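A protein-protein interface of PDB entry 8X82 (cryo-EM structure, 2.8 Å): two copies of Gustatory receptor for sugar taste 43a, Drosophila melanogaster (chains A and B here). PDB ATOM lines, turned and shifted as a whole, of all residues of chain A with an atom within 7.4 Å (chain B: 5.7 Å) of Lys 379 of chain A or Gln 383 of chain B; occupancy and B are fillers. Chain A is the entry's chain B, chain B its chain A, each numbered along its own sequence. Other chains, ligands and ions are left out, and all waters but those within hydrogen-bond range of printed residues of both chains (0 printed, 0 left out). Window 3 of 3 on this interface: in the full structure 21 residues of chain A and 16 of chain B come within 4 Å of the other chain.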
ATOM      1  N   LEU A 271       8.003 -19.911  -4.875  1.00  0.00           N
ATOM      2  CA  LEU A 271       9.254 -19.414  -4.309  1.00  0.00           C
ATOM      3  C   LEU A 271       9.915 -18.389  -5.217  1.00  0.00           C
ATOM      4  O   LEU A 271      10.508 -17.421  -4.729  1.00  0.00           O
ATOM      5  CB  LEU A 271      10.219 -20.567  -4.044  1.00  0.00           C
ATOM      6  CG  LEU A 271      11.467 -20.144  -3.266  1.00  0.00           C
ATOM      7  CD1 LEU A 271      11.218 -20.138  -1.766  1.00  0.00           C
ATOM      8  CD2 LEU A 271      12.642 -21.027  -3.617  1.00  0.00           C
ATOM      9  N   ILE A 359      16.927 -14.367   5.051  1.00  0.00           N
ATOM     10  CA  ILE A 359      18.013 -15.283   4.718  1.00  0.00           C
ATOM     11  C   ILE A 359      18.091 -16.428   5.721  1.00  0.00           C
ATOM     12  O   ILE A 359      18.420 -17.560   5.349  1.00  0.00           O
ATOM     13  CB  ILE A 359      19.347 -14.517   4.606  1.00  0.00           C
ATOM     14  CG1 ILE A 359      20.427 -15.413   3.994  1.00  0.00           C
ATOM     15  CG2 ILE A 359      19.786 -13.965   5.956  1.00  0.00           C
ATOM     16  CD1 ILE A 359      21.637 -14.658   3.508  1.00  0.00           C
ATOM     17  N   VAL A 362      15.402 -18.795   4.700  1.00  0.00           N
ATOM     18  CA  VAL A 362      15.828 -19.524   3.511  1.00  0.00           C
ATOM     19  C   VAL A 362      16.883 -20.571   3.854  1.00  0.00           C
ATOM     20  O   VAL A 362      16.908 -21.650   3.252  1.00  0.00           O
ATOM     21  CB  VAL A 362      16.323 -18.535   2.444  1.00  0.00           C
ATOM     22  CG1 VAL A 362      17.114 -19.246   1.358  1.00  0.00           C
ATOM     23  CG2 VAL A 362      15.143 -17.796   1.845  1.00  0.00           C
ATOM     24  N   CYS A 363      17.765 -20.282   4.814  1.00  0.00           N
ATOM     25  CA  CYS A 363      18.732 -21.284   5.252  1.00  0.00           C
ATOM     26  C   CYS A 363      18.029 -22.504   5.835  1.00  0.00           C
ATOM     27  O   CYS A 363      18.421 -23.646   5.563  1.00  0.00           O
ATOM     28  CB  CYS A 363      19.692 -20.676   6.275  1.00  0.00           C
ATOM     29  SG  CYS A 363      21.063 -19.748   5.552  1.00  0.00           S
ATOM     30  N   GLU A 366      16.675 -24.456   2.967  1.00  0.00           N
ATOM     31  CA  GLU A 366      17.758 -25.240   2.379  1.00  0.00           C
ATOM     32  C   GLU A 366      17.988 -26.523   3.166  1.00  0.00           C
ATOM     33  O   GLU A 366      18.193 -27.598   2.591  1.00  0.00           O
ATOM     34  CB  GLU A 366      19.048 -24.415   2.331  1.00  0.00           C
ATOM     35  CG  GLU A 366      19.185 -23.505   1.125  1.00  0.00           C
ATOM     36  CD  GLU A 366      20.529 -22.805   1.073  1.00  0.00           C
ATOM     37  OE1 GLU A 366      21.274 -22.868   2.073  1.00  0.00           O
ATOM     38  OE2 GLU A 366      20.845 -22.195   0.028  1.00  0.00           O
ATOM     39  N   VAL A 369      14.837 -28.748   2.255  1.00  0.00           N
ATOM     40  CA  VAL A 369      14.434 -29.009   0.876  1.00  0.00           C
ATOM     41  C   VAL A 369      15.198 -30.218   0.350  1.00  0.00           C
ATOM     42  O   VAL A 369      16.348 -30.459   0.737  1.00  0.00           O
ATOM     43  CB  VAL A 369      14.658 -27.774  -0.021  1.00  0.00           C
ATOM     44  CG1 VAL A 369      16.145 -27.521  -0.240  1.00  0.00           C
ATOM     45  CG2 VAL A 369      13.931 -27.930  -1.347  1.00  0.00           C
ATOM     46  N   ILE A 373      14.664 -29.166  -8.415  1.00  0.00           N
ATOM     47  CA  ILE A 373      14.339 -27.832  -8.909  1.00  0.00           C
ATOM     48  C   ILE A 373      14.031 -26.891  -7.748  1.00  0.00           C
ATOM     49  O   ILE A 373      14.410 -25.713  -7.769  1.00  0.00           O
ATOM     50  CB  ILE A 373      13.177 -27.899  -9.918  1.00  0.00           C
ATOM     51  CG1 ILE A 373      11.934 -28.531  -9.286  1.00  0.00           C
ATOM     52  CG2 ILE A 373      13.597 -28.670 -11.162  1.00  0.00           C
ATOM     53  CD1 ILE A 373      10.705 -28.481 -10.168  1.00  0.00           C
ATOM     54  N   LEU A 374      13.350 -27.395  -6.716  1.00  0.00           N
ATOM     55  CA  LEU A 374      13.066 -26.568  -5.549  1.00  0.00           C
ATOM     56  C   LEU A 374      14.349 -26.182  -4.823  1.00  0.00           C
ATOM     57  O   LEU A 374      14.517 -25.024  -4.425  1.00  0.00           O
ATOM     58  CB  LEU A 374      12.110 -27.298  -4.607  1.00  0.00           C
ATOM     59  CG  LEU A 374      11.382 -26.425  -3.584  1.00  0.00           C
ATOM     60  CD1 LEU A 374      10.486 -25.424  -4.287  1.00  0.00           C
ATOM     61  CD2 LEU A 374      10.574 -27.285  -2.627  1.00  0.00           C
ATOM     62  N   ALA A 375      15.271 -27.134  -4.652  1.00  0.00           N
ATOM     63  CA  ALA A 375      16.532 -26.826  -3.984  1.00  0.00           C
ATOM     64  C   ALA A 375      17.347 -25.819  -4.783  1.00  0.00           C
ATOM     65  O   ALA A 375      17.994 -24.938  -4.205  1.00  0.00           O
ATOM     66  CB  ALA A 375      17.340 -28.103  -3.752  1.00  0.00           C
ATOM     67  N   GLU A 376      17.338 -25.939  -6.113  1.00  0.00           N
ATOM     68  CA  GLU A 376      18.022 -24.953  -6.940  1.00  0.00           C
ATOM     69  C   GLU A 376      17.406 -23.568  -6.786  1.00  0.00           C
ATOM     70  O   GLU A 376      18.136 -22.571  -6.713  1.00  0.00           O
ATOM     71  CB  GLU A 376      17.996 -25.386  -8.405  1.00  0.00           C
ATOM     72  CG  GLU A 376      18.628 -24.387  -9.362  1.00  0.00           C
ATOM     73  CD  GLU A 376      20.137 -24.328  -9.232  1.00  0.00           C
ATOM     74  OE1 GLU A 376      20.633 -23.635  -8.320  1.00  0.00           O
ATOM     75  OE2 GLU A 376      20.829 -24.976 -10.045  1.00  0.00           O
ATOM     76  N   ALA A 377      16.075 -23.486  -6.733  1.00  0.00           N
ATOM     77  CA  ALA A 377      15.419 -22.197  -6.541  1.00  0.00           C
ATOM     78  C   ALA A 377      15.771 -21.596  -5.184  1.00  0.00           C
ATOM     79  O   ALA A 377      16.011 -20.388  -5.070  1.00  0.00           O
ATOM     80  CB  ALA A 377      13.906 -22.354  -6.695  1.00  0.00           C
ATOM     81  N   VAL A 378      15.809 -22.429  -4.140  1.00  0.00           N
ATOM     82  CA  VAL A 378      16.170 -21.936  -2.813  1.00  0.00           C
ATOM     83  C   VAL A 378      17.626 -21.491  -2.788  1.00  0.00           C
ATOM     84  O   VAL A 378      17.983 -20.517  -2.115  1.00  0.00           O
ATOM     85  CB  VAL A 378      15.885 -23.004  -1.739  1.00  0.00           C
ATOM     86  CG1 VAL A 378      16.200 -22.460  -0.364  1.00  0.00           C
ATOM     87  CG2 VAL A 378      14.440 -23.446  -1.795  1.00  0.00           C
ATOM     88  N   LYS A 379      18.492 -22.200  -3.518  1.00  0.00           N
ATOM     89  CA  LYS A 379      19.886 -21.783  -3.628  1.00  0.00           C
ATOM     90  C   LYS A 379      19.998 -20.419  -4.298  1.00  0.00           C
ATOM     91  O   LYS A 379      20.787 -19.569  -3.869  1.00  0.00           O
ATOM     92  CB  LYS A 379      20.683 -22.833  -4.403  1.00  0.00           C
ATOM     93  CG  LYS A 379      22.143 -22.479  -4.652  1.00  0.00           C
ATOM     94  CD  LYS A 379      22.836 -21.974  -3.399  1.00  0.00           C
ATOM     95  CE  LYS A 379      24.212 -22.596  -3.249  1.00  0.00           C
ATOM     96  NZ  LYS A 379      25.248 -21.573  -2.935  1.00  0.00           N
ATOM     97  N   LYS A 380      19.212 -20.193  -5.352  1.00  0.00           N
ATOM     98  CA  LYS A 380      19.209 -18.890  -6.010  1.00  0.00           C
ATOM     99  C   LYS A 380      18.729 -17.800  -5.059  1.00  0.00           C
ATOM    100  O   LYS A 380      19.290 -16.699  -5.022  1.00  0.00           O
ATOM    101  CB  LYS A 380      18.331 -18.940  -7.261  1.00  0.00           C
ATOM    102  CG  LYS A 380      18.974 -19.622  -8.454  1.00  0.00           C
ATOM    103  CD  LYS A 380      20.229 -18.893  -8.901  1.00  0.00           C
ATOM    104  CE  LYS A 380      20.749 -19.457 -10.212  1.00  0.00           C
ATOM    105  NZ  LYS A 380      19.770 -19.287 -11.322  1.00  0.00           N
ATOM    106  N   PHE A 381      17.681 -18.093  -4.284  1.00  0.00           N
ATOM    107  CA  PHE A 381      17.172 -17.117  -3.326  1.00  0.00           C
ATOM    108  C   PHE A 381      18.211 -16.797  -2.257  1.00  0.00           C
ATOM    109  O   PHE A 381      18.400 -15.628  -1.899  1.00  0.00           O
ATOM    110  CB  PHE A 381      15.880 -17.640  -2.694  1.00  0.00           C
ATOM    111  CG  PHE A 381      15.042 -16.576  -2.037  1.00  0.00           C
ATOM    112  CD1 PHE A 381      15.360 -15.234  -2.171  1.00  0.00           C
ATOM    113  CD2 PHE A 381      13.923 -16.920  -1.300  1.00  0.00           C
ATOM    114  CE1 PHE A 381      14.588 -14.261  -1.569  1.00  0.00           C
ATOM    115  CE2 PHE A 381      13.147 -15.951  -0.697  1.00  0.00           C
ATOM    116  CZ  PHE A 381      13.478 -14.621  -0.832  1.00  0.00           C
ATOM    117  N   TRP A 382      18.898 -17.817  -1.742  1.00  0.00           N
ATOM    118  CA  TRP A 382      19.934 -17.585  -0.739  1.00  0.00           C
ATOM    119  C   TRP A 382      21.069 -16.745  -1.312  1.00  0.00           C
ATOM    120  O   TRP A 382      21.591 -15.842  -0.647  1.00  0.00           O
ATOM    121  CB  TRP A 382      20.464 -18.919  -0.214  1.00  0.00           C
ATOM    122  CG  TRP A 382      21.458 -18.772   0.896  1.00  0.00           C
ATOM    123  CD1 TRP A 382      21.188 -18.640   2.225  1.00  0.00           C
ATOM    124  CD2 TRP A 382      22.883 -18.731   0.769  1.00  0.00           C
ATOM    125  NE1 TRP A 382      22.357 -18.525   2.937  1.00  0.00           N
ATOM    126  CE2 TRP A 382      23.413 -18.577   2.065  1.00  0.00           C
ATOM    127  CE3 TRP A 382      23.764 -18.812  -0.312  1.00  0.00           C
ATOM    128  CZ2 TRP A 382      24.781 -18.501   2.308  1.00  0.00           C
ATOM    129  CZ3 TRP A 382      25.124 -18.737  -0.070  1.00  0.00           C
ATOM    130  CH2 TRP A 382      25.619 -18.584   1.230  1.00  0.00           C
ATOM    131  N   GLN A 383      21.461 -17.030  -2.555  1.00  0.00           N
ATOM    132  CA  GLN A 383      22.500 -16.241  -3.205  1.00  0.00           C
ATOM    133  C   GLN A 383      22.080 -14.786  -3.362  1.00  0.00           C
ATOM    134  O   GLN A 383      22.895 -13.879  -3.163  1.00  0.00           O
ATOM    135  CB  GLN A 383      22.835 -16.846  -4.567  1.00  0.00           C
ATOM    136  CG  GLN A 383      24.244 -16.564  -5.038  1.00  0.00           C
ATOM    137  CD  GLN A 383      24.948 -17.808  -5.531  1.00  0.00           C
ATOM    138  OE1 GLN A 383      24.683 -18.914  -5.062  1.00  0.00           O
ATOM    139  NE2 GLN A 383      25.851 -17.632  -6.486  1.00  0.00           N
ATOM    140  N   GLN A 384      20.818 -14.547  -3.725  1.00  0.00           N
ATOM    141  CA  GLN A 384      20.321 -13.179  -3.830  1.00  0.00           C
ATOM    142  C   GLN A 384      20.322 -12.483  -2.474  1.00  0.00           C
ATOM    143  O   GLN A 384      20.696 -11.309  -2.371  1.00  0.00           O
ATOM    144  CB  GLN A 384      18.921 -13.183  -4.438  1.00  0.00           C
ATOM    145  CG  GLN A 384      18.123 -11.918  -4.189  1.00  0.00           C
ATOM    146  CD  GLN A 384      16.634 -12.130  -4.371  1.00  0.00           C
ATOM    147  OE1 GLN A 384      15.820 -11.524  -3.676  1.00  0.00           O
ATOM    148  NE2 GLN A 384      16.271 -12.996  -5.309  1.00  0.00           N
ATOM    149  N   LEU A 385      19.915 -13.193  -1.421  1.00  0.00           N
ATOM    150  CA  LEU A 385      19.855 -12.612  -0.086  1.00  0.00           C
ATOM    151  C   LEU A 385      21.228 -12.407   0.535  1.00  0.00           C
ATOM    152  O   LEU A 385      21.329 -11.749   1.576  1.00  0.00           O
ATOM    153  CB  LEU A 385      19.012 -13.494   0.836  1.00  0.00           C
ATOM    154  CG  LEU A 385      17.541 -13.624   0.455  1.00  0.00           C
ATOM    155  CD1 LEU A 385      16.906 -14.755   1.226  1.00  0.00           C
ATOM    156  CD2 LEU A 385      16.812 -12.325   0.711  1.00  0.00           C
ATOM    157  N   LEU A 386      22.280 -12.969  -0.060  1.00  0.00           N
ATOM    158  CA  LEU A 386      23.620 -12.764   0.478  1.00  0.00           C
ATOM    159  C   LEU A 386      24.054 -11.306   0.397  1.00  0.00           C
ATOM    160  O   LEU A 386      24.761 -10.822   1.289  1.00  0.00           O
ATOM    161  CB  LEU A 386      24.623 -13.649  -0.263  1.00  0.00           C
ATOM    162  CG  LEU A 386      25.888 -14.053   0.497  1.00  0.00           C
ATOM    163  CD1 LEU A 386      25.627 -14.148   1.991  1.00  0.00           C
ATOM    164  CD2 LEU A 386      26.439 -15.362  -0.040  1.00  0.00           C
ATOM    165  N   VAL B 378      29.269 -30.903   5.738  1.00  0.00           N
ATOM    166  CA  VAL B 378      30.144 -29.822   6.190  1.00  0.00           C
ATOM    167  C   VAL B 378      29.941 -28.579   5.336  1.00  0.00           C
ATOM    168  O   VAL B 378      30.007 -27.447   5.831  1.00  0.00           O
ATOM    169  CB  VAL B 378      31.616 -30.278   6.189  1.00  0.00           C
ATOM    170  CG1 VAL B 378      32.505 -29.176   6.720  1.00  0.00           C
ATOM    171  CG2 VAL B 378      31.791 -31.525   7.026  1.00  0.00           C
ATOM    172  N   LYS B 379      29.695 -28.766   4.036  1.00  0.00           N
ATOM    173  CA  LYS B 379      29.393 -27.634   3.166  1.00  0.00           C
ATOM    174  C   LYS B 379      28.107 -26.939   3.602  1.00  0.00           C
ATOM    175  O   LYS B 379      28.033 -25.705   3.616  1.00  0.00           O
ATOM    176  CB  LYS B 379      29.286 -28.107   1.716  1.00  0.00           C
ATOM    177  CG  LYS B 379      28.898 -27.028   0.714  1.00  0.00           C
ATOM    178  CD  LYS B 379      29.705 -25.755   0.896  1.00  0.00           C
ATOM    179  CE  LYS B 379      30.167 -25.207  -0.443  1.00  0.00           C
ATOM    180  NZ  LYS B 379      29.904 -23.746  -0.561  1.00  0.00           N
ATOM    181  N   LYS B 380      27.085 -27.719   3.962  1.00  0.00           N
ATOM    182  CA  LYS B 380      25.843 -27.134   4.455  1.00  0.00           C
ATOM    183  C   LYS B 380      26.080 -26.360   5.746  1.00  0.00           C
ATOM    184  O   LYS B 380      25.538 -25.265   5.940  1.00  0.00           O
ATOM    185  CB  LYS B 380      24.798 -28.230   4.667  1.00  0.00           C
ATOM    186  CG  LYS B 380      24.143 -28.727   3.391  1.00  0.00           C
ATOM    187  CD  LYS B 380      23.388 -27.616   2.684  1.00  0.00           C
ATOM    188  CE  LYS B 380      22.570 -28.164   1.528  1.00  0.00           C
ATOM    189  NZ  LYS B 380      21.529 -29.127   1.985  1.00  0.00           N
ATOM    190  N   PHE B 381      26.887 -26.923   6.648  1.00  0.00           N
ATOM    191  CA  PHE B 381      27.190 -26.241   7.903  1.00  0.00           C
ATOM    192  C   PHE B 381      27.939 -24.936   7.656  1.00  0.00           C
ATOM    193  O   PHE B 381      27.634 -23.912   8.278  1.00  0.00           O
ATOM    194  CB  PHE B 381      27.995 -27.169   8.815  1.00  0.00           C
ATOM    195  CG  PHE B 381      27.991 -26.761  10.265  1.00  0.00           C
ATOM    196  CD1 PHE B 381      27.177 -25.735  10.715  1.00  0.00           C
ATOM    197  CD2 PHE B 381      28.793 -27.419  11.180  1.00  0.00           C
ATOM    198  CE1 PHE B 381      27.176 -25.365  12.045  1.00  0.00           C
ATOM    199  CE2 PHE B 381      28.794 -27.055  12.511  1.00  0.00           C
ATOM    200  CZ  PHE B 381      27.985 -26.028  12.945  1.00  0.00           C
ATOM    201  N   TRP B 382      28.916 -24.951   6.749  1.00  0.00           N
ATOM    202  CA  TRP B 382      29.655 -23.730   6.432  1.00  0.00           C
ATOM    203  C   TRP B 382      28.733 -22.675   5.834  1.00  0.00           C
ATOM    204  O   TRP B 382      28.832 -21.486   6.162  1.00  0.00           O
ATOM    205  CB  TRP B 382      30.804 -24.047   5.476  1.00  0.00           C
ATOM    206  CG  TRP B 382      31.678 -22.868   5.182  1.00  0.00           C
ATOM    207  CD1 TRP B 382      32.741 -22.433   5.916  1.00  0.00           C
ATOM    208  CD2 TRP B 382      31.558 -21.967   4.075  1.00  0.00           C
ATOM    209  NE1 TRP B 382      33.294 -21.318   5.334  1.00  0.00           N
ATOM    210  CE2 TRP B 382      32.585 -21.012   4.203  1.00  0.00           C
ATOM    211  CE3 TRP B 382      30.683 -21.876   2.989  1.00  0.00           C
ATOM    212  CZ2 TRP B 382      32.761 -19.978   3.287  1.00  0.00           C
ATOM    213  CZ3 TRP B 382      30.860 -20.850   2.079  1.00  0.00           C
ATOM    214  CH2 TRP B 382      31.891 -19.915   2.233  1.00  0.00           C
ATOM    215  N   GLN B 383      27.826 -23.097   4.952  1.00  0.00           N
ATOM    216  CA  GLN B 383      26.866 -22.166   4.371  1.00  0.00           C
ATOM    217  C   GLN B 383      25.969 -21.555   5.439  1.00  0.00           C
ATOM    218  O   GLN B 383      25.668 -20.358   5.386  1.00  0.00           O
ATOM    219  CB  GLN B 383      26.023 -22.881   3.317  1.00  0.00           C
ATOM    220  CG  GLN B 383      25.484 -21.970   2.237  1.00  0.00           C
ATOM    221  CD  GLN B 383      25.718 -22.517   0.848  1.00  0.00           C
ATOM    222  OE1 GLN B 383      26.697 -23.223   0.602  1.00  0.00           O
ATOM    223  NE2 GLN B 383      24.820 -22.194  -0.072  1.00  0.00           N
ATOM    224  N   GLN B 384      25.526 -22.361   6.406  1.00  0.00           N
ATOM    225  CA  GLN B 384      24.718 -21.836   7.500  1.00  0.00           C
ATOM    226  C   GLN B 384      25.509 -20.847   8.348  1.00  0.00           C
ATOM    227  O   GLN B 384      24.984 -19.800   8.745  1.00  0.00           O
ATOM    228  CB  GLN B 384      24.193 -22.987   8.355  1.00  0.00           C
ATOM    229  CG  GLN B 384      23.739 -22.584   9.744  1.00  0.00           C
ATOM    230  CD  GLN B 384      23.685 -23.758  10.697  1.00  0.00           C
ATOM    231  OE1 GLN B 384      23.955 -23.618  11.889  1.00  0.00           O
ATOM    232  NE2 GLN B 384      23.337 -24.928  10.176  1.00  0.00           N
ATOM    233  N   LEU B 385      26.775 -21.156   8.629  1.00  0.00           N
ATOM    234  CA  LEU B 385      27.608 -20.290   9.453  1.00  0.00           C
ATOM    235  C   LEU B 385      28.038 -19.020   8.735  1.00  0.00           C
ATOM    236  O   LEU B 385      28.581 -18.116   9.377  1.00  0.00           O
ATOM    237  CB  LEU B 385      28.849 -21.046   9.925  1.00  0.00           C
ATOM    238  CG  LEU B 385      28.584 -22.236  10.843  1.00  0.00           C
ATOM    239  CD1 LEU B 385      29.829 -23.079  10.970  1.00  0.00           C
ATOM    240  CD2 LEU B 385      28.118 -21.762  12.201  1.00  0.00           C
ATOM    241  N   LEU B 386      27.830 -18.939   7.421  1.00  0.00           N
ATOM    242  CA  LEU B 386      28.191 -17.723   6.698  1.00  0.00           C
ATOM    243  C   LEU B 386      27.360 -16.526   7.143  1.00  0.00           C
ATOM    244  O   LEU B 386      27.870 -15.400   7.178  1.00  0.00           O
ATOM    245  CB  LEU B 386      28.029 -17.941   5.194  1.00  0.00           C
ATOM    246  CG  LEU B 386      28.894 -17.082   4.270  1.00  0.00           C
ATOM    247  CD1 LEU B 386      30.216 -16.724   4.930  1.00  0.00           C
ATOM    248  CD2 LEU B 386      29.125 -17.789   2.946  1.00  0.00           C
ATOM    249  N   VAL B 387      26.091 -16.739   7.488  1.00  0.00           N
ATOM    250  CA  VAL B 387      25.161 -15.633   7.692  1.00  0.00           C
ATOM    251  C   VAL B 387      24.549 -15.653   9.089  1.00  0.00           C
ATOM    252  O   VAL B 387      23.426 -15.179   9.290  1.00  0.00           O
ATOM    253  CB  VAL B 387      24.059 -15.656   6.615  1.00  0.00           C
ATOM    254  CG1 VAL B 387      24.678 -15.560   5.235  1.00  0.00           C
ATOM    255  CG2 VAL B 387      23.230 -16.929   6.728  1.00  0.00           C
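Among the printed residues, merely in contact across the chains: Ile 359 of chain A with Val 387 of chain B (3.6 Å), Cys 363 of chain A with Val 387 of chain B (3.7 Å), Glu 366 of chain A with Lys 380 of chain B (3.7 Å), Glu 366 of chain A with Gln 383 of chain B (3.98 Å), Trp 382 of chain A with Gln 383 of chain B (3.5 Å), Trp 382 of chain A with Leu 386 of chain B (3.98 Å) and Leu 386 of chain A with Val 387 of chain B (3.7 Å).
Lys 379 of chain A touches Gln 383 of chain B, but with the chains exchanged Gln 383 of chain A does not touch Lys 379 of chain B (8.4 Å). Trp 382 of chain A touches Gln 383 of chain B, but with the chains exchanged Gln 383 of chain A does not touch Trp 382 of chain B (9.6 Å). Trp 382 of chain A touches Leu 386 of chain B, but with the chains exchanged Leu 386 of chain A does not touch Trp 382 of chain B (7.4 Å). Positions printed for both chains: 378, 379, 380, 381, 382, 383, 384, 385 and 386. Of the 8 pairs that touch across the chains among the printed residues, none has its exchanged pair printed and touching as well.
Of chain B, only Gln 383 (3.0 Å) comes within 4 Å of Lys 379 of chain A. Gln 383 of chain B touches just these residues of chain A: Glu 366 (3.98 Å), Lys 379 (3.0 Å) and Trp 382 (3.5 Å). Of the printed residues of chain B, Trp 382 of chain A touches Gln 383 (3.5 Å) and Leu 386 (3.98 Å). Printed residues of chain A within 4 Å of Val 387 of chain B: Ile 359 (3.6 Å), Cys 363 (3.7 Å) and Leu 386 (3.7 Å). Of the printed residues of chain B, Cys 363 of chain A touches Val 387 (3.7 Å). Of the printed residues of chain A, Lys 380 of chain B touches Glu 366 (3.7 Å). Printed residues of chain A within 4 Å of Leu 386 of chain B: Trp 382 (3.98 Å). Leu 385 of chain B touches none of the printed residues of chain A. The nearest printed residue of chain B that does not touch Lys 379 of chain A is Lys 379 of chain B (5.7 Å). The nearest printed residue of chain B that does not touch Trp 382 of chain A is Val 387 of chain B (4.2 Å).
Of the 20 printed residues of chain A, 6 touch a printed residue of chain B. Hydrophobic or aromatic side chains of chain A within 4 Å of the printed part of chain B: Ile 359, Trp 382 and Leu 386. Of the 10 printed residues of chain B, 4 touch a printed residue of chain A. Among the printed residues, 8 pairs touch across the chains.
NE2 of Gln 383 of chain B sits close to NZ of Lys 379 of chain A, at 3.0 Å.
The side-chain amino group of Lys 379 of chain B is in hydrogen-bond range of the side-chain amide oxygen of Gln 383 of chain B. The side-chain sulfur (SG) of Cys 363 of chain A is in hydrogen-bond range of the backbone carbonyl oxygen (O) of Ile 359 of chain A. The indole nitrogen (NE1) of Trp 382 of chain A is in hydrogen-bond range of the side-chain sulfur (SG) of Cys 363 of chain A. The side-chain amide oxygen (OE1) of Gln 383 of chain A is in hydrogen-bond range of the side-chain amino group (NZ) of Lys 379 of chain A, at 3.5 Å.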
